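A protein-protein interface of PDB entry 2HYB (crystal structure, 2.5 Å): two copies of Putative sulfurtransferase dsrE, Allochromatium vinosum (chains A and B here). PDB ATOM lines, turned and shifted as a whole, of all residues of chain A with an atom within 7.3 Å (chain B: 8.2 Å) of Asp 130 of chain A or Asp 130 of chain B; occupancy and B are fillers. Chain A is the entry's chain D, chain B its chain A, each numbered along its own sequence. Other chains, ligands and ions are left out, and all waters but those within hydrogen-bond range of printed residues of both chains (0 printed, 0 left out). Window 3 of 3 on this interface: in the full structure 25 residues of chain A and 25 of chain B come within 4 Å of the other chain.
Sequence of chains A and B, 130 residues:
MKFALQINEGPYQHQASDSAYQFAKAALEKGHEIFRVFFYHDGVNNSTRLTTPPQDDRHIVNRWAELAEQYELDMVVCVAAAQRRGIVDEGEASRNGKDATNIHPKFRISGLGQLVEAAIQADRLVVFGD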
ATOM      1  N   ASN A   8      -2.985 -24.018  18.862  1.00  0.00           N
ATOM      2  CA  ASN A   8      -3.851 -24.078  20.032  1.00  0.00           C
ATOM      3  C   ASN A   8      -4.214 -22.791  20.721  1.00  0.00           C
ATOM      4  O   ASN A   8      -5.005 -22.805  21.668  1.00  0.00           O
ATOM      5  CB  ASN A   8      -3.251 -25.016  21.084  1.00  0.00           C
ATOM      6  CG  ASN A   8      -2.849 -26.362  20.509  1.00  0.00           C
ATOM      7  OD1 ASN A   8      -3.465 -26.852  19.557  1.00  0.00           O
ATOM      8  ND2 ASN A   8      -1.816 -26.969  21.088  1.00  0.00           N
ATOM      9  N   GLU A   9      -3.670 -21.669  20.278  1.00  0.00           N
ATOM     10  CA  GLU A   9      -4.001 -20.435  20.970  1.00  0.00           C
ATOM     11  C   GLU A   9      -4.607 -19.365  20.074  1.00  0.00           C
ATOM     12  O   GLU A   9      -4.476 -19.397  18.853  1.00  0.00           O
ATOM     13  CB  GLU A   9      -2.756 -19.915  21.678  1.00  0.00           C
ATOM     14  CG  GLU A   9      -2.108 -20.944  22.602  1.00  0.00           C
ATOM     15  CD  GLU A   9      -3.031 -21.432  23.723  1.00  0.00           C
ATOM     16  OE1 GLU A   9      -3.822 -20.624  24.273  1.00  0.00           O
ATOM     17  OE2 GLU A   9      -2.946 -22.628  24.072  1.00  0.00           O
ATOM     18  N   GLN A  13      -2.765 -12.890  22.061  1.00  0.00           N
ATOM     19  CA  GLN A  13      -2.633 -13.264  23.465  1.00  0.00           C
ATOM     20  C   GLN A  13      -1.381 -14.122  23.666  1.00  0.00           C
ATOM     21  O   GLN A  13      -0.655 -13.962  24.655  1.00  0.00           O
ATOM     22  CB  GLN A  13      -3.890 -14.034  23.906  1.00  0.00           C
ATOM     23  CG  GLN A  13      -3.982 -14.331  25.382  1.00  0.00           C
ATOM     24  CD  GLN A  13      -4.611 -13.203  26.176  1.00  0.00           C
ATOM     25  OE1 GLN A  13      -4.800 -12.105  25.667  1.00  0.00           O
ATOM     26  NE2 GLN A  13      -4.938 -13.473  27.434  1.00  0.00           N
ATOM     27  N   HIS A  14      -1.135 -15.028  22.721  1.00  0.00           N
ATOM     28  CA  HIS A  14       0.022 -15.920  22.770  1.00  0.00           C
ATOM     29  C   HIS A  14       0.682 -15.879  21.399  1.00  0.00           C
ATOM     30  O   HIS A  14      -0.001 -15.737  20.392  1.00  0.00           O
ATOM     31  CB  HIS A  14      -0.391 -17.367  23.099  1.00  0.00           C
ATOM     32  CG  HIS A  14      -0.989 -17.548  24.465  1.00  0.00           C
ATOM     33  ND1 HIS A  14      -2.344 -17.450  24.707  1.00  0.00           N
ATOM     34  CD2 HIS A  14      -0.419 -17.831  25.662  1.00  0.00           C
ATOM     35  CE1 HIS A  14      -2.585 -17.668  25.990  1.00  0.00           C
ATOM     36  NE2 HIS A  14      -1.433 -17.902  26.593  1.00  0.00           N
ATOM     37  N   ALA A  16       2.026 -18.254  19.681  1.00  0.00           N
ATOM     38  CA  ALA A  16       1.761 -19.451  18.878  1.00  0.00           C
ATOM     39  C   ALA A  16       1.352 -19.231  17.412  1.00  0.00           C
ATOM     40  O   ALA A  16       2.005 -19.744  16.501  1.00  0.00           O
ATOM     41  CB  ALA A  16       0.707 -20.336  19.587  1.00  0.00           C
ATOM     42  N   PHE A 128       1.982 -25.715  17.701  1.00  0.00           N
ATOM     43  CA  PHE A 128       2.305 -24.419  18.271  1.00  0.00           C
ATOM     44  C   PHE A 128       1.271 -24.024  19.322  1.00  0.00           C
ATOM     45  O   PHE A 128       0.117 -23.732  18.986  1.00  0.00           O
ATOM     46  CB  PHE A 128       2.292 -23.352  17.186  1.00  0.00           C
ATOM     47  CG  PHE A 128       3.305 -23.558  16.105  1.00  0.00           C
ATOM     48  CD1 PHE A 128       3.000 -24.323  14.984  1.00  0.00           C
ATOM     49  CD2 PHE A 128       4.573 -22.975  16.212  1.00  0.00           C
ATOM     50  CE1 PHE A 128       3.946 -24.500  13.979  1.00  0.00           C
ATOM     51  CE2 PHE A 128       5.517 -23.145  15.228  1.00  0.00           C
ATOM     52  CZ  PHE A 128       5.211 -23.910  14.101  1.00  0.00           C
ATOM     53  N   GLY A 129       1.676 -23.985  20.588  1.00  0.00           N
ATOM     54  CA  GLY A 129       0.736 -23.609  21.626  1.00  0.00           C
ATOM     55  C   GLY A 129       1.360 -22.809  22.750  1.00  0.00           C
ATOM     56  O   GLY A 129       2.347 -22.087  22.562  1.00  0.00           O
ATOM     57  N   ASP A 130       0.773 -22.950  23.933  1.00  0.00           N
ATOM     58  CA  ASP A 130       1.226 -22.259  25.134  1.00  0.00           C
ATOM     59  C   ASP A 130       2.351 -23.059  25.790  1.00  0.00           C
ATOM     60  O   ASP A 130       2.101 -24.015  26.516  1.00  0.00           O
ATOM     61  CB  ASP A 130       0.043 -22.109  26.102  1.00  0.00           C
ATOM     62  CG  ASP A 130       0.251 -21.014  27.125  1.00  0.00           C
ATOM     63  OD1 ASP A 130      -0.701 -20.713  27.879  1.00  0.00           O
ATOM     64  OD2 ASP A 130       1.360 -20.452  27.184  1.00  0.00           O
ATOM     65  N   ILE B   7     -10.918  -9.640  34.886  1.00  0.00           N
ATOM     66  CA  ILE B   7     -10.790 -10.956  34.260  1.00  0.00           C
ATOM     67  C   ILE B   7      -9.987 -10.838  32.973  1.00  0.00           C
ATOM     68  O   ILE B   7     -10.444 -10.215  32.008  1.00  0.00           O
ATOM     69  CB  ILE B   7     -12.173 -11.522  33.938  1.00  0.00           C
ATOM     70  CG1 ILE B   7     -13.055 -11.418  35.178  1.00  0.00           C
ATOM     71  CG2 ILE B   7     -12.059 -12.968  33.483  1.00  0.00           C
ATOM     72  CD1 ILE B   7     -14.456 -11.965  34.978  1.00  0.00           C
ATOM     73  N   ASN B   8      -8.804 -11.451  32.947  1.00  0.00           N
ATOM     74  CA  ASN B   8      -7.927 -11.351  31.774  1.00  0.00           C
ATOM     75  C   ASN B   8      -7.957 -12.501  30.790  1.00  0.00           C
ATOM     76  O   ASN B   8      -7.235 -12.470  29.799  1.00  0.00           O
ATOM     77  CB  ASN B   8      -6.469 -11.171  32.197  1.00  0.00           C
ATOM     78  CG  ASN B   8      -6.296 -10.161  33.300  1.00  0.00           C
ATOM     79  OD1 ASN B   8      -6.953  -9.116  33.315  1.00  0.00           O
ATOM     80  ND2 ASN B   8      -5.390 -10.455  34.225  1.00  0.00           N
ATOM     81  N   GLU B   9      -8.764 -13.519  31.039  1.00  0.00           N
ATOM     82  CA  GLU B   9      -8.775 -14.638  30.110  1.00  0.00           C
ATOM     83  C   GLU B   9     -10.132 -14.969  29.511  1.00  0.00           C
ATOM     84  O   GLU B   9     -11.180 -14.566  30.022  1.00  0.00           O
ATOM     85  CB  GLU B   9      -8.218 -15.885  30.790  1.00  0.00           C
ATOM     86  CG  GLU B   9      -6.881 -15.694  31.501  1.00  0.00           C
ATOM     87  CD  GLU B   9      -5.715 -15.380  30.570  1.00  0.00           C
ATOM     88  OE1 GLU B   9      -5.664 -15.909  29.432  1.00  0.00           O
ATOM     89  OE2 GLU B   9      -4.833 -14.615  31.008  1.00  0.00           O
ATOM     90  N   GLN B  13     -11.136 -21.815  28.145  1.00  0.00           N
ATOM     91  CA  GLN B  13      -9.705 -22.061  27.984  1.00  0.00           C
ATOM     92  C   GLN B  13      -8.973 -22.051  29.324  1.00  0.00           C
ATOM     93  O   GLN B  13      -8.135 -22.918  29.590  1.00  0.00           O
ATOM     94  CB  GLN B  13      -9.084 -21.020  27.054  1.00  0.00           C
ATOM     95  CG  GLN B  13      -7.648 -21.312  26.652  1.00  0.00           C
ATOM     96  CD  GLN B  13      -7.553 -22.203  25.431  1.00  0.00           C
ATOM     97  OE1 GLN B  13      -8.546 -22.799  25.011  1.00  0.00           O
ATOM     98  NE2 GLN B  13      -6.355 -22.301  24.853  1.00  0.00           N
ATOM     99  N   HIS B  14      -9.287 -21.062  30.157  1.00  0.00           N
ATOM    100  CA  HIS B  14      -8.683 -20.918  31.476  1.00  0.00           C
ATOM    101  C   HIS B  14      -9.823 -20.825  32.489  1.00  0.00           C
ATOM    102  O   HIS B  14     -10.929 -20.401  32.141  1.00  0.00           O
ATOM    103  CB  HIS B  14      -7.817 -19.645  31.545  1.00  0.00           C
ATOM    104  CG  HIS B  14      -6.621 -19.664  30.632  1.00  0.00           C
ATOM    105  ND1 HIS B  14      -6.640 -19.134  29.359  1.00  0.00           N
ATOM    106  CD2 HIS B  14      -5.364 -20.131  30.824  1.00  0.00           C
ATOM    107  CE1 HIS B  14      -5.448 -19.271  28.807  1.00  0.00           C
ATOM    108  NE2 HIS B  14      -4.655 -19.872  29.675  1.00  0.00           N
ATOM    109  N   GLN B  15      -9.567 -21.207  33.736  1.00  0.00           N
ATOM    110  CA  GLN B  15     -10.609 -21.175  34.764  1.00  0.00           C
ATOM    111  C   GLN B  15     -10.946 -19.775  35.261  1.00  0.00           C
ATOM    112  O   GLN B  15     -12.015 -19.547  35.826  1.00  0.00           O
ATOM    113  CB  GLN B  15     -10.202 -22.047  35.955  1.00  0.00           C
ATOM    114  CG  GLN B  15     -11.368 -22.542  36.809  1.00  0.00           C
ATOM    115  CD  GLN B  15     -10.899 -23.298  38.055  1.00  0.00           C
ATOM    116  OE1 GLN B  15      -9.809 -23.893  38.062  1.00  0.00           O
ATOM    117  NE2 GLN B  15     -11.722 -23.287  39.109  1.00  0.00           N
ATOM    118  N   ALA B  16     -10.017 -18.849  35.067  1.00  0.00           N
ATOM    119  CA  ALA B  16     -10.195 -17.466  35.500  1.00  0.00           C
ATOM    120  C   ALA B  16     -11.645 -16.963  35.578  1.00  0.00           C
ATOM    121  O   ALA B  16     -12.134 -16.631  36.662  1.00  0.00           O
ATOM    122  CB  ALA B  16      -9.373 -16.527  34.593  1.00  0.00           C
ATOM    123  N   SER B  17     -12.322 -16.906  34.429  1.00  0.00           N
ATOM    124  CA  SER B  17     -13.689 -16.392  34.355  1.00  0.00           C
ATOM    125  C   SER B  17     -14.656 -17.092  35.301  1.00  0.00           C
ATOM    126  O   SER B  17     -15.457 -16.442  35.979  1.00  0.00           O
ATOM    127  CB  SER B  17     -14.204 -16.482  32.918  1.00  0.00           C
ATOM    128  OG  SER B  17     -15.447 -15.820  32.782  1.00  0.00           O
ATOM    129  N   HIS B  41      -7.649  -8.133  27.955  1.00  0.00           N
ATOM    130  CA  HIS B  41      -6.980  -9.247  27.266  1.00  0.00           C
ATOM    131  C   HIS B  41      -8.051 -10.205  26.728  1.00  0.00           C
ATOM    132  O   HIS B  41      -9.183  -9.798  26.459  1.00  0.00           O
ATOM    133  CB  HIS B  41      -6.086 -10.043  28.223  1.00  0.00           C
ATOM    134  CG  HIS B  41      -5.077  -9.219  28.963  1.00  0.00           C
ATOM    135  ND1 HIS B  41      -3.993  -8.632  28.351  1.00  0.00           N
ATOM    136  CD2 HIS B  41      -4.980  -8.909  30.278  1.00  0.00           C
ATOM    137  CE1 HIS B  41      -3.269  -7.995  29.256  1.00  0.00           C
ATOM    138  NE2 HIS B  41      -3.848  -8.150  30.434  1.00  0.00           N
ATOM    139  N   VAL B 127      -8.014  -9.580  40.973  1.00  0.00           N
ATOM    140  CA  VAL B 127      -7.663  -9.941  39.605  1.00  0.00           C
ATOM    141  C   VAL B 127      -7.600 -11.453  39.302  1.00  0.00           C
ATOM    142  O   VAL B 127      -6.856 -12.201  39.948  1.00  0.00           O
ATOM    143  CB  VAL B 127      -6.308  -9.308  39.242  1.00  0.00           C
ATOM    144  CG1 VAL B 127      -5.873  -9.751  37.863  1.00  0.00           C
ATOM    145  CG2 VAL B 127      -6.409  -7.800  39.317  1.00  0.00           C
ATOM    146  N   PHE B 128      -8.368 -11.888  38.301  1.00  0.00           N
ATOM    147  CA  PHE B 128      -8.395 -13.292  37.894  1.00  0.00           C
ATOM    148  C   PHE B 128      -7.764 -13.490  36.514  1.00  0.00           C
ATOM    149  O   PHE B 128      -8.189 -12.881  35.525  1.00  0.00           O
ATOM    150  CB  PHE B 128      -9.836 -13.814  37.884  1.00  0.00           C
ATOM    151  CG  PHE B 128     -10.512 -13.770  39.229  1.00  0.00           C
ATOM    152  CD1 PHE B 128     -11.060 -12.588  39.707  1.00  0.00           C
ATOM    153  CD2 PHE B 128     -10.604 -14.908  40.017  1.00  0.00           C
ATOM    154  CE1 PHE B 128     -11.691 -12.538  40.948  1.00  0.00           C
ATOM    155  CE2 PHE B 128     -11.230 -14.872  41.260  1.00  0.00           C
ATOM    156  CZ  PHE B 128     -11.777 -13.686  41.728  1.00  0.00           C
ATOM    157  N   GLY B 129      -6.749 -14.347  36.444  1.00  0.00           N
ATOM    158  CA  GLY B 129      -6.082 -14.588  35.173  1.00  0.00           C
ATOM    159  C   GLY B 129      -5.367 -15.926  35.052  1.00  0.00           C
ATOM    160  O   GLY B 129      -5.760 -16.920  35.668  1.00  0.00           O
ATOM    161  N   ASP B 130      -4.306 -15.944  34.253  1.00  0.00           N
ATOM    162  CA  ASP B 130      -3.526 -17.148  34.023  1.00  0.00           C
ATOM    163  C   ASP B 130      -2.433 -17.255  35.092  1.00  0.00           C
ATOM    164  O   ASP B 130      -1.268 -16.943  34.841  1.00  0.00           O
ATOM    165  CB  ASP B 130      -2.910 -17.094  32.617  1.00  0.00           C
ATOM    166  CG  ASP B 130      -2.461 -18.456  32.114  1.00  0.00           C
ATOM    167  OD1 ASP B 130      -2.091 -18.566  30.920  1.00  0.00           O
ATOM    168  OD2 ASP B 130      -2.477 -19.416  32.916  1.00  0.00           O
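Asp 130 of chain A touches just one residue of chain B: Asp 130. Of chain A, only Asp 130 (3.97 Å) comes within 4 Å of Asp 130 of chain B. No residue of chain B comes within 4 Å of Gly 129 of chain A. Printed residues of chain A within 4 Å of His 41 of chain B: Gln 13 (3.5 Å). Printed residues of chain B within 4 Å of Gln 13 of chain A: Asn 8 (3.4 Å), Glu 9 (3.2 Å) and His 41 (3.5 Å). Of the printed residues of chain B, Asn 8 of chain A touches Gln 13 (3.5 Å). Ala 16 of chain A touches none of the printed residues of chain B. Ser 17 of chain B touches none of the printed residues of chain A.
Asn 8 of chain A touches Gln 13 of chain B, and with the chains exchanged Gln 13 of chain A touches Asn 8 of chain B. Glu 9 of chain A touches Gln 13 of chain B, and with the chains exchanged Gln 13 of chain A touches Glu 9 of chain B. Asp 130 of chain B touches its own counterpart, Asp 130 of chain A. Of the 6 pairs that touch across the chains among the printed residues, 5 have their exchanged pair printed and touching as well.
Printed residues of chain A that touch a printed residue of chain B: Asn 8, Glu 9, Gln 13 and Asp 130. Of the 13 printed residues of chain B, 5 touch a printed residue of chain A. Among the printed residues, no Asp or Glu carboxylate lies within 4 Å of a Lys or Arg side-chain nitrogen of the other chain.
The backbone NH (N) of Asn 8 of chain B lies within hydrogen-bond range of the backbone carbonyl oxygen (O) of Phe 128 of chain B (3.0 Å). ND1 of His 14 of chain B is in hydrogen-bond range of OE1 of Glu 9 of chain B, 3.4 Å away. A ring nitrogen (NE2) of His 14 of chain B sits at hydrogen-bond distance from the side-chain carboxylate (OD1) of Asp 130 of chain B. The backbone NH (N) of Asn 8 of chain A sits at hydrogen-bond distance from the backbone carbonyl oxygen (O) of Phe 128 of chain A. NE2 of His 14 of chain A is in hydrogen-bond range of OD1 of Asp 130 of chain A (3.2 Å).
The side-chain amide nitrogen (NE2) of Gln 13 of chain A lies within hydrogen-bond range of the backbone carbonyl oxygen (O) of Asn 8 of chain B (3.4 Å). The side-chain carboxylate (OE1) of Glu 9 of chain B is in hydrogen-bond range of the side-chain amide nitrogen (NE2) of Gln 13 of chain A (3.2 Å). NE2 of Gln 13 of chain B sits at hydrogen-bond distance from O of Asn 8 of chain A (3.5 Å). The side-chain carboxylate (OE1) of Glu 9 of chain A sits at hydrogen-bond distance from the side-chain amide nitrogen (NE2) of Gln 13 of chain B.
His 41 of chain B touches Gln 13 of chain A (CB to OE1, 3.5 Å). OD1 of Asp 130 of chain A touches OD1 of Asp 130 of chain B, at 3.97 Å.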
